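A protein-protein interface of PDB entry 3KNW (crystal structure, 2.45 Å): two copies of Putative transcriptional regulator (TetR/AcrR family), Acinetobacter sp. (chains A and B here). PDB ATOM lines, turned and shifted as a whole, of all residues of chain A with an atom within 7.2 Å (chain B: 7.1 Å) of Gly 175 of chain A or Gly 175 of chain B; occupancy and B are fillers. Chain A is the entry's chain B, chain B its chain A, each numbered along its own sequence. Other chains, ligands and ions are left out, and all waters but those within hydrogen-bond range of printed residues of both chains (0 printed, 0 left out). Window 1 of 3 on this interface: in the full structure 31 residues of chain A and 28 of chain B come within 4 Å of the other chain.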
ATOM      1  N   TRP A  98      16.464  33.284 -18.874  1.00  0.00           N
ATOM      2  CA  TRP A  98      17.738  32.611 -18.455  1.00  0.00           C
ATOM      3  C   TRP A  98      18.971  32.967 -19.289  1.00  0.00           C
ATOM      4  O   TRP A  98      20.131  32.684 -18.917  1.00  0.00           O
ATOM      5  CB  TRP A  98      17.620  31.082 -18.595  1.00  0.00           C
ATOM      6  CG  TRP A  98      16.758  30.376 -17.601  1.00  0.00           C
ATOM      7  CD1 TRP A  98      15.406  30.500 -17.431  1.00  0.00           C
ATOM      8  CD2 TRP A  98      17.211  29.456 -16.626  1.00  0.00           C
ATOM      9  NE1 TRP A  98      14.989  29.682 -16.410  1.00  0.00           N
ATOM     10  CE2 TRP A  98      16.079  29.031 -15.896  1.00  0.00           C
ATOM     11  CE3 TRP A  98      18.461  28.933 -16.304  1.00  0.00           C
ATOM     12  CZ2 TRP A  98      16.167  28.108 -14.878  1.00  0.00           C
ATOM     13  CZ3 TRP A  98      18.538  27.999 -15.318  1.00  0.00           C
ATOM     14  CH2 TRP A  98      17.397  27.597 -14.608  1.00  0.00           C
ATOM     15  N   ILE A 114      21.337  28.372  -7.459  1.00  0.00           N
ATOM     16  CA  ILE A 114      21.071  26.940  -7.226  1.00  0.00           C
ATOM     17  C   ILE A 114      22.414  26.176  -7.254  1.00  0.00           C
ATOM     18  O   ILE A 114      22.648  25.318  -6.417  1.00  0.00           O
ATOM     19  CB  ILE A 114      20.037  26.337  -8.191  1.00  0.00           C
ATOM     20  CG1 ILE A 114      18.676  26.948  -7.951  1.00  0.00           C
ATOM     21  CG2 ILE A 114      19.853  24.835  -7.954  1.00  0.00           C
ATOM     22  CD1 ILE A 114      17.572  26.160  -8.603  1.00  0.00           C
ATOM     23  N   ILE A 169      12.607  19.835 -18.785  1.00  0.00           N
ATOM     24  CA  ILE A 169      12.984  21.169 -19.192  1.00  0.00           C
ATOM     25  C   ILE A 169      13.808  21.775 -18.090  1.00  0.00           C
ATOM     26  O   ILE A 169      14.889  22.342 -18.378  1.00  0.00           O
ATOM     27  CB  ILE A 169      11.859  22.052 -19.483  1.00  0.00           C
ATOM     28  CG1 ILE A 169      11.187  21.600 -20.779  1.00  0.00           C
ATOM     29  CG2 ILE A 169      12.338  23.493 -19.621  1.00  0.00           C
ATOM     30  CD1 ILE A 169       9.853  22.318 -21.032  1.00  0.00           C
ATOM     31  N   TYR A 170      13.379  21.599 -16.828  1.00  0.00           N
ATOM     32  CA  TYR A 170      14.079  22.366 -15.792  1.00  0.00           C
ATOM     33  C   TYR A 170      15.488  21.827 -15.569  1.00  0.00           C
ATOM     34  O   TYR A 170      16.436  22.583 -15.430  1.00  0.00           O
ATOM     35  CB  TYR A 170      13.275  22.419 -14.505  1.00  0.00           C
ATOM     36  CG  TYR A 170      13.869  23.362 -13.471  1.00  0.00           C
ATOM     37  CD1 TYR A 170      13.754  24.739 -13.588  1.00  0.00           C
ATOM     38  CD2 TYR A 170      14.559  22.864 -12.380  1.00  0.00           C
ATOM     39  CE1 TYR A 170      14.342  25.613 -12.637  1.00  0.00           C
ATOM     40  CE2 TYR A 170      15.143  23.718 -11.435  1.00  0.00           C
ATOM     41  CZ  TYR A 170      15.036  25.090 -11.554  1.00  0.00           C
ATOM     42  OH  TYR A 170      15.649  25.903 -10.567  1.00  0.00           O
ATOM     43  N   GLN A 171      15.632  20.521 -15.541  1.00  0.00           N
ATOM     44  CA  GLN A 171      16.901  19.944 -15.382  1.00  0.00           C
ATOM     45  C   GLN A 171      17.816  20.334 -16.531  1.00  0.00           C
ATOM     46  O   GLN A 171      18.995  20.618 -16.294  1.00  0.00           O
ATOM     47  CB  GLN A 171      16.812  18.418 -15.282  1.00  0.00           C
ATOM     48  CG  GLN A 171      16.234  17.895 -13.956  1.00  0.00           C
ATOM     49  CD  GLN A 171      15.926  16.406 -14.018  1.00  0.00           C
ATOM     50  OE1 GLN A 171      16.242  15.733 -14.978  1.00  0.00           O
ATOM     51  NE2 GLN A 171      15.318  15.904 -12.996  1.00  0.00           N
ATOM     52  N   MET A 172      17.292  20.341 -17.761  1.00  0.00           N
ATOM     53  CA  MET A 172      18.106  20.697 -18.954  1.00  0.00           C
ATOM     54  C   MET A 172      18.680  22.076 -18.758  1.00  0.00           C
ATOM     55  O   MET A 172      19.899  22.302 -18.939  1.00  0.00           O
ATOM     56  CB  MET A 172      17.265  20.648 -20.243  1.00  0.00           C
ATOM     57  CG  MET A 172      18.076  20.755 -21.549  1.00  0.00           C
ATOM     58  SD  MET A 172      17.090  20.421 -23.089  1.00  0.00           S
ATOM     59  CE  MET A 172      15.744  21.689 -22.764  1.00  0.00           C
ATOM     60  N   TYR A 173      17.834  22.999 -18.286  1.00  0.00           N
ATOM     61  CA  TYR A 173      18.295  24.395 -18.173  1.00  0.00           C
ATOM     62  C   TYR A 173      19.327  24.548 -17.086  1.00  0.00           C
ATOM     63  O   TYR A 173      20.277  25.270 -17.283  1.00  0.00           O
ATOM     64  CB  TYR A 173      17.176  25.393 -17.990  1.00  0.00           C
ATOM     65  CG  TYR A 173      16.592  25.779 -19.261  1.00  0.00           C
ATOM     66  CD1 TYR A 173      15.824  24.889 -19.941  1.00  0.00           C
ATOM     67  CD2 TYR A 173      16.883  27.019 -19.857  1.00  0.00           C
ATOM     68  CE1 TYR A 173      15.291  25.180 -21.170  1.00  0.00           C
ATOM     69  CE2 TYR A 173      16.322  27.360 -21.066  1.00  0.00           C
ATOM     70  CZ  TYR A 173      15.527  26.418 -21.743  1.00  0.00           C
ATOM     71  OH  TYR A 173      14.941  26.658 -22.985  1.00  0.00           O
ATOM     72  N   LEU A 174      19.175  23.887 -15.950  1.00  0.00           N
ATOM     73  CA  LEU A 174      20.206  23.944 -14.864  1.00  0.00           C
ATOM     74  C   LEU A 174      21.487  23.393 -15.364  1.00  0.00           C
ATOM     75  O   LEU A 174      22.536  23.929 -15.149  1.00  0.00           O
ATOM     76  CB  LEU A 174      19.805  23.117 -13.675  1.00  0.00           C
ATOM     77  CG  LEU A 174      18.651  23.599 -12.805  1.00  0.00           C
ATOM     78  CD1 LEU A 174      18.416  22.623 -11.640  1.00  0.00           C
ATOM     79  CD2 LEU A 174      18.900  25.016 -12.271  1.00  0.00           C
ATOM     80  N   GLY A 175      21.437  22.349 -16.129  1.00  0.00           N
ATOM     81  CA  GLY A 175      22.703  21.828 -16.695  1.00  0.00           C
ATOM     82  C   GLY A 175      23.351  22.721 -17.745  1.00  0.00           C
ATOM     83  O   GLY A 175      24.590  22.953 -17.683  1.00  0.00           O
ATOM     84  N   ALA A 176      22.540  23.206 -18.705  1.00  0.00           N
ATOM     85  CA  ALA A 176      22.987  24.253 -19.657  1.00  0.00           C
ATOM     86  C   ALA A 176      23.590  25.481 -18.879  1.00  0.00           C
ATOM     87  O   ALA A 176      24.692  25.987 -19.197  1.00  0.00           O
ATOM     88  CB  ALA A 176      21.811  24.681 -20.561  1.00  0.00           C
ATOM     89  N   ALA A 177      22.938  25.896 -17.783  1.00  0.00           N
ATOM     90  CA  ALA A 177      23.482  27.056 -17.069  1.00  0.00           C
ATOM     91  C   ALA A 177      24.814  26.707 -16.386  1.00  0.00           C
ATOM     92  O   ALA A 177      25.780  27.485 -16.345  1.00  0.00           O
ATOM     93  CB  ALA A 177      22.466  27.616 -16.119  1.00  0.00           C
ATOM     94  N   LEU A 178      24.964  25.489 -15.952  1.00  0.00           N
ATOM     95  CA  LEU A 178      26.224  25.119 -15.294  1.00  0.00           C
ATOM     96  C   LEU A 178      27.300  25.150 -16.322  1.00  0.00           C
ATOM     97  O   LEU A 178      28.378  25.659 -16.094  1.00  0.00           O
ATOM     98  CB  LEU A 178      26.149  23.671 -14.735  1.00  0.00           C
ATOM     99  CG  LEU A 178      26.591  23.416 -13.300  1.00  0.00           C
ATOM    100  CD1 LEU A 178      26.101  24.535 -12.424  1.00  0.00           C
ATOM    101  CD2 LEU A 178      26.035  22.121 -12.815  1.00  0.00           C
ATOM    102  N   LEU A 179      27.036  24.550 -17.465  1.00  0.00           N
ATOM    103  CA  LEU A 179      28.063  24.500 -18.529  1.00  0.00           C
ATOM    104  C   LEU A 179      28.309  25.877 -19.085  1.00  0.00           C
ATOM    105  O   LEU A 179      29.428  26.186 -19.381  1.00  0.00           O
ATOM    106  CB  LEU A 179      27.646  23.570 -19.682  1.00  0.00           C
ATOM    107  CG  LEU A 179      27.683  22.071 -19.435  1.00  0.00           C
ATOM    108  CD1 LEU A 179      27.186  21.329 -20.668  1.00  0.00           C
ATOM    109  CD2 LEU A 179      29.117  21.569 -19.064  1.00  0.00           C
ATOM    110  N   SER A 180      27.293  26.750 -19.201  1.00  0.00           N
ATOM    111  CA  SER A 180      27.569  28.188 -19.605  1.00  0.00           C
ATOM    112  C   SER A 180      28.512  28.896 -18.654  1.00  0.00           C
ATOM    113  O   SER A 180      29.422  29.594 -19.066  1.00  0.00           O
ATOM    114  CB  SER A 180      26.297  28.999 -19.736  1.00  0.00           C
ATOM    115  OG  SER A 180      25.391  28.300 -20.584  1.00  0.00           O
ATOM    116  N   LYS A 181      28.325  28.723 -17.375  1.00  0.00           N
ATOM    117  CA  LYS A 181      29.219  29.337 -16.399  1.00  0.00           C
ATOM    118  C   LYS A 181      30.622  28.873 -16.615  1.00  0.00           C
ATOM    119  O   LYS A 181      31.567  29.633 -16.574  1.00  0.00           O
ATOM    120  CB  LYS A 181      28.791  28.989 -14.968  1.00  0.00           C
ATOM    121  CG  LYS A 181      28.131  30.113 -14.244  1.00  0.00           C
ATOM    122  CD  LYS A 181      27.679  29.752 -12.764  1.00  0.00           C
ATOM    123  CE  LYS A 181      28.704  30.164 -11.667  1.00  0.00           C
ATOM    124  NZ  LYS A 181      28.314  29.681 -10.253  1.00  0.00           N
ATOM    125  N   PRO A 188      25.590  26.605 -24.458  1.00  0.00           N
ATOM    126  CA  PRO A 188      24.665  25.558 -23.907  1.00  0.00           C
ATOM    127  C   PRO A 188      23.229  25.991 -23.739  1.00  0.00           C
ATOM    128  O   PRO A 188      22.310  25.248 -24.067  1.00  0.00           O
ATOM    129  CB  PRO A 188      25.232  25.289 -22.558  1.00  0.00           C
ATOM    130  CG  PRO A 188      26.745  25.481 -22.726  1.00  0.00           C
ATOM    131  CD  PRO A 188      26.891  26.594 -23.795  1.00  0.00           C
ATOM    132  N   LEU A 189      23.024  27.186 -23.205  1.00  0.00           N
ATOM    133  CA  LEU A 189      21.691  27.679 -23.012  1.00  0.00           C
ATOM    134  C   LEU A 189      21.032  28.007 -24.358  1.00  0.00           C
ATOM    135  O   LEU A 189      19.843  27.764 -24.511  1.00  0.00           O
ATOM    136  CB  LEU A 189      21.693  28.828 -22.064  1.00  0.00           C
ATOM    137  CG  LEU A 189      21.714  28.481 -20.557  1.00  0.00           C
ATOM    138  CD1 LEU A 189      22.216  29.707 -19.735  1.00  0.00           C
ATOM    139  CD2 LEU A 189      20.335  27.957 -20.080  1.00  0.00           C
ATOM    140  N   TRP B  98      26.136   6.770 -13.801  1.00  0.00           N
ATOM    141  CA  TRP B  98      25.960   8.123 -13.290  1.00  0.00           C
ATOM    142  C   TRP B  98      25.107   8.056 -12.040  1.00  0.00           C
ATOM    143  O   TRP B  98      25.499   8.535 -11.008  1.00  0.00           O
ATOM    144  CB  TRP B  98      25.200   8.977 -14.301  1.00  0.00           C
ATOM    145  CG  TRP B  98      25.879  10.079 -14.972  1.00  0.00           C
ATOM    146  CD1 TRP B  98      26.535  10.031 -16.156  1.00  0.00           C
ATOM    147  CD2 TRP B  98      25.861  11.447 -14.581  1.00  0.00           C
ATOM    148  NE1 TRP B  98      26.983  11.284 -16.509  1.00  0.00           N
ATOM    149  CE2 TRP B  98      26.578  12.173 -15.558  1.00  0.00           C
ATOM    150  CE3 TRP B  98      25.339  12.123 -13.491  1.00  0.00           C
ATOM    151  CZ2 TRP B  98      26.783  13.531 -15.469  1.00  0.00           C
ATOM    152  CZ3 TRP B  98      25.534  13.450 -13.409  1.00  0.00           C
ATOM    153  CH2 TRP B  98      26.259  14.153 -14.388  1.00  0.00           C
ATOM    154  N   ILE B 114      31.908  18.796 -11.265  1.00  0.00           N
ATOM    155  CA  ILE B 114      31.539  19.878 -12.189  1.00  0.00           C
ATOM    156  C   ILE B 114      30.707  20.937 -11.490  1.00  0.00           C
ATOM    157  O   ILE B 114      30.785  22.100 -11.854  1.00  0.00           O
ATOM    158  CB  ILE B 114      30.802  19.408 -13.464  1.00  0.00           C
ATOM    159  CG1 ILE B 114      31.782  18.860 -14.477  1.00  0.00           C
ATOM    160  CG2 ILE B 114      30.128  20.548 -14.157  1.00  0.00           C
ATOM    161  CD1 ILE B 114      31.087  18.158 -15.617  1.00  0.00           C
ATOM    162  N   GLN B 167      23.895  16.620 -26.022  1.00  0.00           N
ATOM    163  CA  GLN B 167      23.871  17.805 -25.154  1.00  0.00           C
ATOM    164  C   GLN B 167      22.629  17.807 -24.259  1.00  0.00           C
ATOM    165  O   GLN B 167      22.709  18.117 -23.059  1.00  0.00           O
ATOM    166  CB  GLN B 167      23.842  19.105 -25.973  1.00  0.00           C
ATOM    167  CG  GLN B 167      25.191  19.535 -26.589  1.00  0.00           C
ATOM    168  CD  GLN B 167      25.040  20.766 -27.475  1.00  0.00           C
ATOM    169  OE1 GLN B 167      24.972  21.935 -26.983  1.00  0.00           O
ATOM    170  NE2 GLN B 167      24.976  20.531 -28.770  1.00  0.00           N
ATOM    171  N   ILE B 169      20.894  15.230 -23.371  1.00  0.00           N
ATOM    172  CA  ILE B 169      21.039  14.199 -22.361  1.00  0.00           C
ATOM    173  C   ILE B 169      22.051  14.639 -21.287  1.00  0.00           C
ATOM    174  O   ILE B 169      21.738  14.627 -20.054  1.00  0.00           O
ATOM    175  CB  ILE B 169      21.442  12.876 -22.979  1.00  0.00           C
ATOM    176  CG1 ILE B 169      20.295  12.300 -23.761  1.00  0.00           C
ATOM    177  CG2 ILE B 169      21.870  11.892 -21.930  1.00  0.00           C
ATOM    178  CD1 ILE B 169      20.721  11.109 -24.584  1.00  0.00           C
ATOM    179  N   TYR B 170      23.212  15.112 -21.725  1.00  0.00           N
ATOM    180  CA  TYR B 170      24.206  15.482 -20.742  1.00  0.00           C
ATOM    181  C   TYR B 170      23.764  16.687 -19.861  1.00  0.00           C
ATOM    182  O   TYR B 170      24.017  16.714 -18.668  1.00  0.00           O
ATOM    183  CB  TYR B 170      25.561  15.707 -21.385  1.00  0.00           C
ATOM    184  CG  TYR B 170      26.660  15.884 -20.382  1.00  0.00           C
ATOM    185  CD1 TYR B 170      27.304  14.802 -19.825  1.00  0.00           C
ATOM    186  CD2 TYR B 170      27.084  17.132 -20.013  1.00  0.00           C
ATOM    187  CE1 TYR B 170      28.361  14.968 -18.912  1.00  0.00           C
ATOM    188  CE2 TYR B 170      28.138  17.295 -19.096  1.00  0.00           C
ATOM    189  CZ  TYR B 170      28.780  16.209 -18.583  1.00  0.00           C
ATOM    190  OH  TYR B 170      29.800  16.383 -17.676  1.00  0.00           O
ATOM    191  N   GLN B 171      23.060  17.635 -20.440  1.00  0.00           N
ATOM    192  CA  GLN B 171      22.595  18.769 -19.680  1.00  0.00           C
ATOM    193  C   GLN B 171      21.572  18.347 -18.658  1.00  0.00           C
ATOM    194  O   GLN B 171      21.664  18.772 -17.543  1.00  0.00           O
ATOM    195  CB  GLN B 171      21.988  19.806 -20.588  1.00  0.00           C
ATOM    196  CG  GLN B 171      23.039  20.643 -21.277  1.00  0.00           C
ATOM    197  CD  GLN B 171      22.490  21.538 -22.346  1.00  0.00           C
ATOM    198  OE1 GLN B 171      23.224  22.075 -23.137  1.00  0.00           O
ATOM    199  NE2 GLN B 171      21.211  21.695 -22.370  1.00  0.00           N
ATOM    200  N   MET B 172      20.620  17.503 -19.033  1.00  0.00           N
ATOM    201  CA  MET B 172      19.579  17.000 -18.130  1.00  0.00           C
ATOM    202  C   MET B 172      20.139  16.200 -17.029  1.00  0.00           C
ATOM    203  O   MET B 172      19.693  16.348 -15.891  1.00  0.00           O
ATOM    204  CB  MET B 172      18.549  16.179 -18.878  1.00  0.00           C
ATOM    205  CG  MET B 172      17.488  15.459 -17.998  1.00  0.00           C
ATOM    206  SD  MET B 172      16.311  14.489 -19.206  1.00  0.00           S
ATOM    207  CE  MET B 172      17.374  12.969 -19.548  1.00  0.00           C
ATOM    208  N   TYR B 173      21.183  15.403 -17.279  1.00  0.00           N
ATOM    209  CA  TYR B 173      21.780  14.669 -16.150  1.00  0.00           C
ATOM    210  C   TYR B 173      22.512  15.543 -15.179  1.00  0.00           C
ATOM    211  O   TYR B 173      22.370  15.364 -13.980  1.00  0.00           O
ATOM    212  CB  TYR B 173      22.653  13.508 -16.607  1.00  0.00           C
ATOM    213  CG  TYR B 173      21.804  12.307 -16.926  1.00  0.00           C
ATOM    214  CD1 TYR B 173      20.985  12.271 -18.067  1.00  0.00           C
ATOM    215  CD2 TYR B 173      21.768  11.211 -16.089  1.00  0.00           C
ATOM    216  CE1 TYR B 173      20.227  11.163 -18.392  1.00  0.00           C
ATOM    217  CE2 TYR B 173      20.977  10.087 -16.429  1.00  0.00           C
ATOM    218  CZ  TYR B 173      20.204  10.095 -17.555  1.00  0.00           C
ATOM    219  OH  TYR B 173      19.416   8.988 -17.843  1.00  0.00           O
ATOM    220  N   LEU B 174      23.272  16.537 -15.639  1.00  0.00           N
ATOM    221  CA  LEU B 174      23.908  17.476 -14.712  1.00  0.00           C
ATOM    222  C   LEU B 174      22.883  18.221 -13.859  1.00  0.00           C
ATOM    223  O   LEU B 174      23.073  18.421 -12.672  1.00  0.00           O
ATOM    224  CB  LEU B 174      24.681  18.492 -15.465  1.00  0.00           C
ATOM    225  CG  LEU B 174      25.983  18.032 -16.102  1.00  0.00           C
ATOM    226  CD1 LEU B 174      26.474  19.143 -17.011  1.00  0.00           C
ATOM    227  CD2 LEU B 174      26.997  17.686 -15.086  1.00  0.00           C
ATOM    228  N   GLY B 175      21.757  18.583 -14.441  1.00  0.00           N
ATOM    229  CA  GLY B 175      20.789  19.322 -13.672  1.00  0.00           C
ATOM    230  C   GLY B 175      20.024  18.447 -12.667  1.00  0.00           C
ATOM    231  O   GLY B 175      19.713  18.921 -11.555  1.00  0.00           O
ATOM    232  N   ALA B 176      19.657  17.228 -13.100  1.00  0.00           N
ATOM    233  CA  ALA B 176      19.216  16.179 -12.218  1.00  0.00           C
ATOM    234  C   ALA B 176      20.280  15.872 -11.075  1.00  0.00           C
ATOM    235  O   ALA B 176      19.921  15.713  -9.919  1.00  0.00           O
ATOM    236  CB  ALA B 176      18.913  14.879 -13.043  1.00  0.00           C
ATOM    237  N   ALA B 177      21.564  15.785 -11.387  1.00  0.00           N
ATOM    238  CA  ALA B 177      22.613  15.562 -10.291  1.00  0.00           C
ATOM    239  C   ALA B 177      22.609  16.734  -9.301  1.00  0.00           C
ATOM    240  O   ALA B 177      22.614  16.530  -8.114  1.00  0.00           O
ATOM    241  CB  ALA B 177      23.978  15.388 -10.843  1.00  0.00           C
ATOM    242  N   LEU B 178      22.506  17.966  -9.812  1.00  0.00           N
ATOM    243  CA  LEU B 178      22.405  19.161  -8.974  1.00  0.00           C
ATOM    244  C   LEU B 178      21.164  19.129  -8.014  1.00  0.00           C
ATOM    245  O   LEU B 178      21.312  19.393  -6.832  1.00  0.00           O
ATOM    246  CB  LEU B 178      22.294  20.360  -9.905  1.00  0.00           C
ATOM    247  CG  LEU B 178      22.726  21.737  -9.511  1.00  0.00           C
ATOM    248  CD1 LEU B 178      22.957  22.597 -10.757  1.00  0.00           C
ATOM    249  CD2 LEU B 178      21.646  22.281  -8.747  1.00  0.00           C
ATOM    250  N   LEU B 179      19.967  18.830  -8.531  1.00  0.00           N
ATOM    251  CA  LEU B 179      18.752  18.749  -7.704  1.00  0.00           C
ATOM    252  C   LEU B 179      18.841  17.629  -6.700  1.00  0.00           C
ATOM    253  O   LEU B 179      18.449  17.782  -5.547  1.00  0.00           O
ATOM    254  CB  LEU B 179      17.483  18.541  -8.549  1.00  0.00           C
ATOM    255  CG  LEU B 179      17.017  19.744  -9.369  1.00  0.00           C
ATOM    256  CD1 LEU B 179      15.623  19.486 -10.001  1.00  0.00           C
ATOM    257  CD2 LEU B 179      16.969  21.048  -8.526  1.00  0.00           C
ATOM    258  N   SER B 180      19.370  16.505  -7.127  1.00  0.00           N
ATOM    259  CA  SER B 180      19.629  15.381  -6.192  1.00  0.00           C
ATOM    260  C   SER B 180      20.487  15.777  -4.965  1.00  0.00           C
ATOM    261  O   SER B 180      20.213  15.373  -3.856  1.00  0.00           O
ATOM    262  CB  SER B 180      20.225  14.167  -6.946  1.00  0.00           C
ATOM    263  OG  SER B 180      19.282  13.741  -7.959  1.00  0.00           O
ATOM    264  N   LYS B 181      21.488  16.596  -5.151  1.00  0.00           N
ATOM    265  CA  LYS B 181      22.223  17.134  -4.007  1.00  0.00           C
ATOM    266  C   LYS B 181      21.370  18.057  -3.135  1.00  0.00           C
ATOM    267  O   LYS B 181      21.413  18.001  -1.900  1.00  0.00           O
ATOM    268  CB  LYS B 181      23.453  17.923  -4.478  1.00  0.00           C
ATOM    269  CG  LYS B 181      24.449  17.087  -5.228  1.00  0.00           C
ATOM    270  CD  LYS B 181      24.696  15.711  -4.505  1.00  0.00           C
ATOM    271  CE  LYS B 181      26.175  15.251  -4.580  1.00  0.00           C
ATOM    272  NZ  LYS B 181      26.326  13.909  -3.933  1.00  0.00           N
ATOM    273  N   PRO B 188      15.404  12.902  -8.753  1.00  0.00           N
ATOM    274  CA  PRO B 188      15.536  13.577 -10.092  1.00  0.00           C
ATOM    275  C   PRO B 188      16.327  12.813 -11.132  1.00  0.00           C
ATOM    276  O   PRO B 188      16.011  12.892 -12.324  1.00  0.00           O
ATOM    277  CB  PRO B 188      16.207  14.904  -9.733  1.00  0.00           C
ATOM    278  CG  PRO B 188      15.781  15.191  -8.355  1.00  0.00           C
ATOM    279  CD  PRO B 188      15.634  13.847  -7.639  1.00  0.00           C
ATOM    280  N   LEU B 189      17.341  12.082 -10.682  1.00  0.00           N
ATOM    281  CA  LEU B 189      18.226  11.256 -11.533  1.00  0.00           C
ATOM    282  C   LEU B 189      17.499  10.011 -11.971  1.00  0.00           C
ATOM    283  O   LEU B 189      17.582   9.631 -13.115  1.00  0.00           O
ATOM    284  CB  LEU B 189      19.500  10.805 -10.790  1.00  0.00           C
ATOM    285  CG  LEU B 189      20.615  11.823 -10.741  1.00  0.00           C
ATOM    286  CD1 LEU B 189      21.667  11.633  -9.626  1.00  0.00           C
ATOM    287  CD2 LEU B 189      21.300  11.877 -12.102  1.00  0.00           C
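O of Ala 176 of chain B is in hydrogen-bond range of OG of Ser 180 of chain B.
O of Ala 176 of chain A is in hydrogen-bond range of OG of Ser 180 of chain A (2.8 Å).
Of the printed residues of chain B, Gly 175 of chain A touches Gln 171 (3.3 Å) and Gly 175 (3.95 Å).
Gly 175 of chain B touches three residues of chain A.
Printed residues of chain A within 4 Å of Leu 179 of chain B: Leu 174 (3.8 Å).
Printed residues of chain A within 4 Å of Pro 188 of chain B: Gln 171.
The nearest residue of chain B that does not touch Gly 175 of chain A is Leu 174 of chain B (4.1 Å).
The nearest residue of chain A that does not touch Gly 175 of chain B is Met 172 of chain A (5.5 Å).
The nearest printed residue of chain B that does not touch Ile 114 of chain A is Leu 179 of chain B (4.8 Å).
Among the printed residues, pairs that only touch across the chains: Ile 114 of chain A with Leu 178 of chain B (3.2 Å), Gln 171 of chain A with Met 172 of chain B (3.3 Å), Gln 171 of chain A with Gly 175 of chain B (3.4 Å), Gln 171 of chain A with Ala 176 of chain B (3.4 Å), Met 172 of chain A with Gln 171 of chain B (3.4 Å), Leu 174 of chain A with Gly 175 of chain B (3.9 Å), Leu 174 of chain A with Leu 179 of chain B (3.8 Å), Gly 175 of chain A with Gln 171 of chain B (3.3 Å), Gly 175 of chain A with Gly 175 of chain B (3.95 Å), Ala 176 of chain A with Gln 171 of chain B (3.5 Å), Leu 178 of chain A with Leu 178 of chain B (3.7 Å) and Leu 179 of chain A with Leu 174 of chain B (3.99 Å).
Ile 114 of chain A touches Leu 178 of chain B, but with the chains exchanged Leu 178 of chain A does not touch Ile 114 of chain B (4.6 Å).
Gln 171 of chain A touches Met 172 of chain B, and with the chains exchanged Met 172 of chain A touches Gln 171 of chain B.
Leu 174 of chain A touches Leu 179 of chain B, and with the chains exchanged Leu 179 of chain A touches Leu 174 of chain B.
Gly 175 of chain B touches its own counterpart, Gly 175 of chain A.
17 positions are printed for both chains.
O of Gln 171 of chain A lies close to O of Gln 171 of chain B (3.5 Å).
The backbone carbonyl oxygen of Pro 188 of chain B lies within hydrogen-bond range of the side-chain amide nitrogen of Gln 171 of chain A, 3.2 Å away.
O of Pro 188 of chain A lies close to OE1 of Gln 171 of chain B.
Hydrophobic or aromatic side chains of chain A that line the printed part of chain B: Ile 114, Met 172, Leu 174, Ala 176, Leu 178, Leu 179 and Pro 188.
Printed residues of chain B that touch a printed residue of chain A: Gln 171, Met 172, Leu 174, Gly 175, Ala 176, Leu 178, Leu 179 and Pro 188.
Hydrophobic or aromatic side chains of chain B that line the printed part of chain A: Met 172, Leu 174, Ala 176, Leu 178, Leu 179 and Pro 188.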
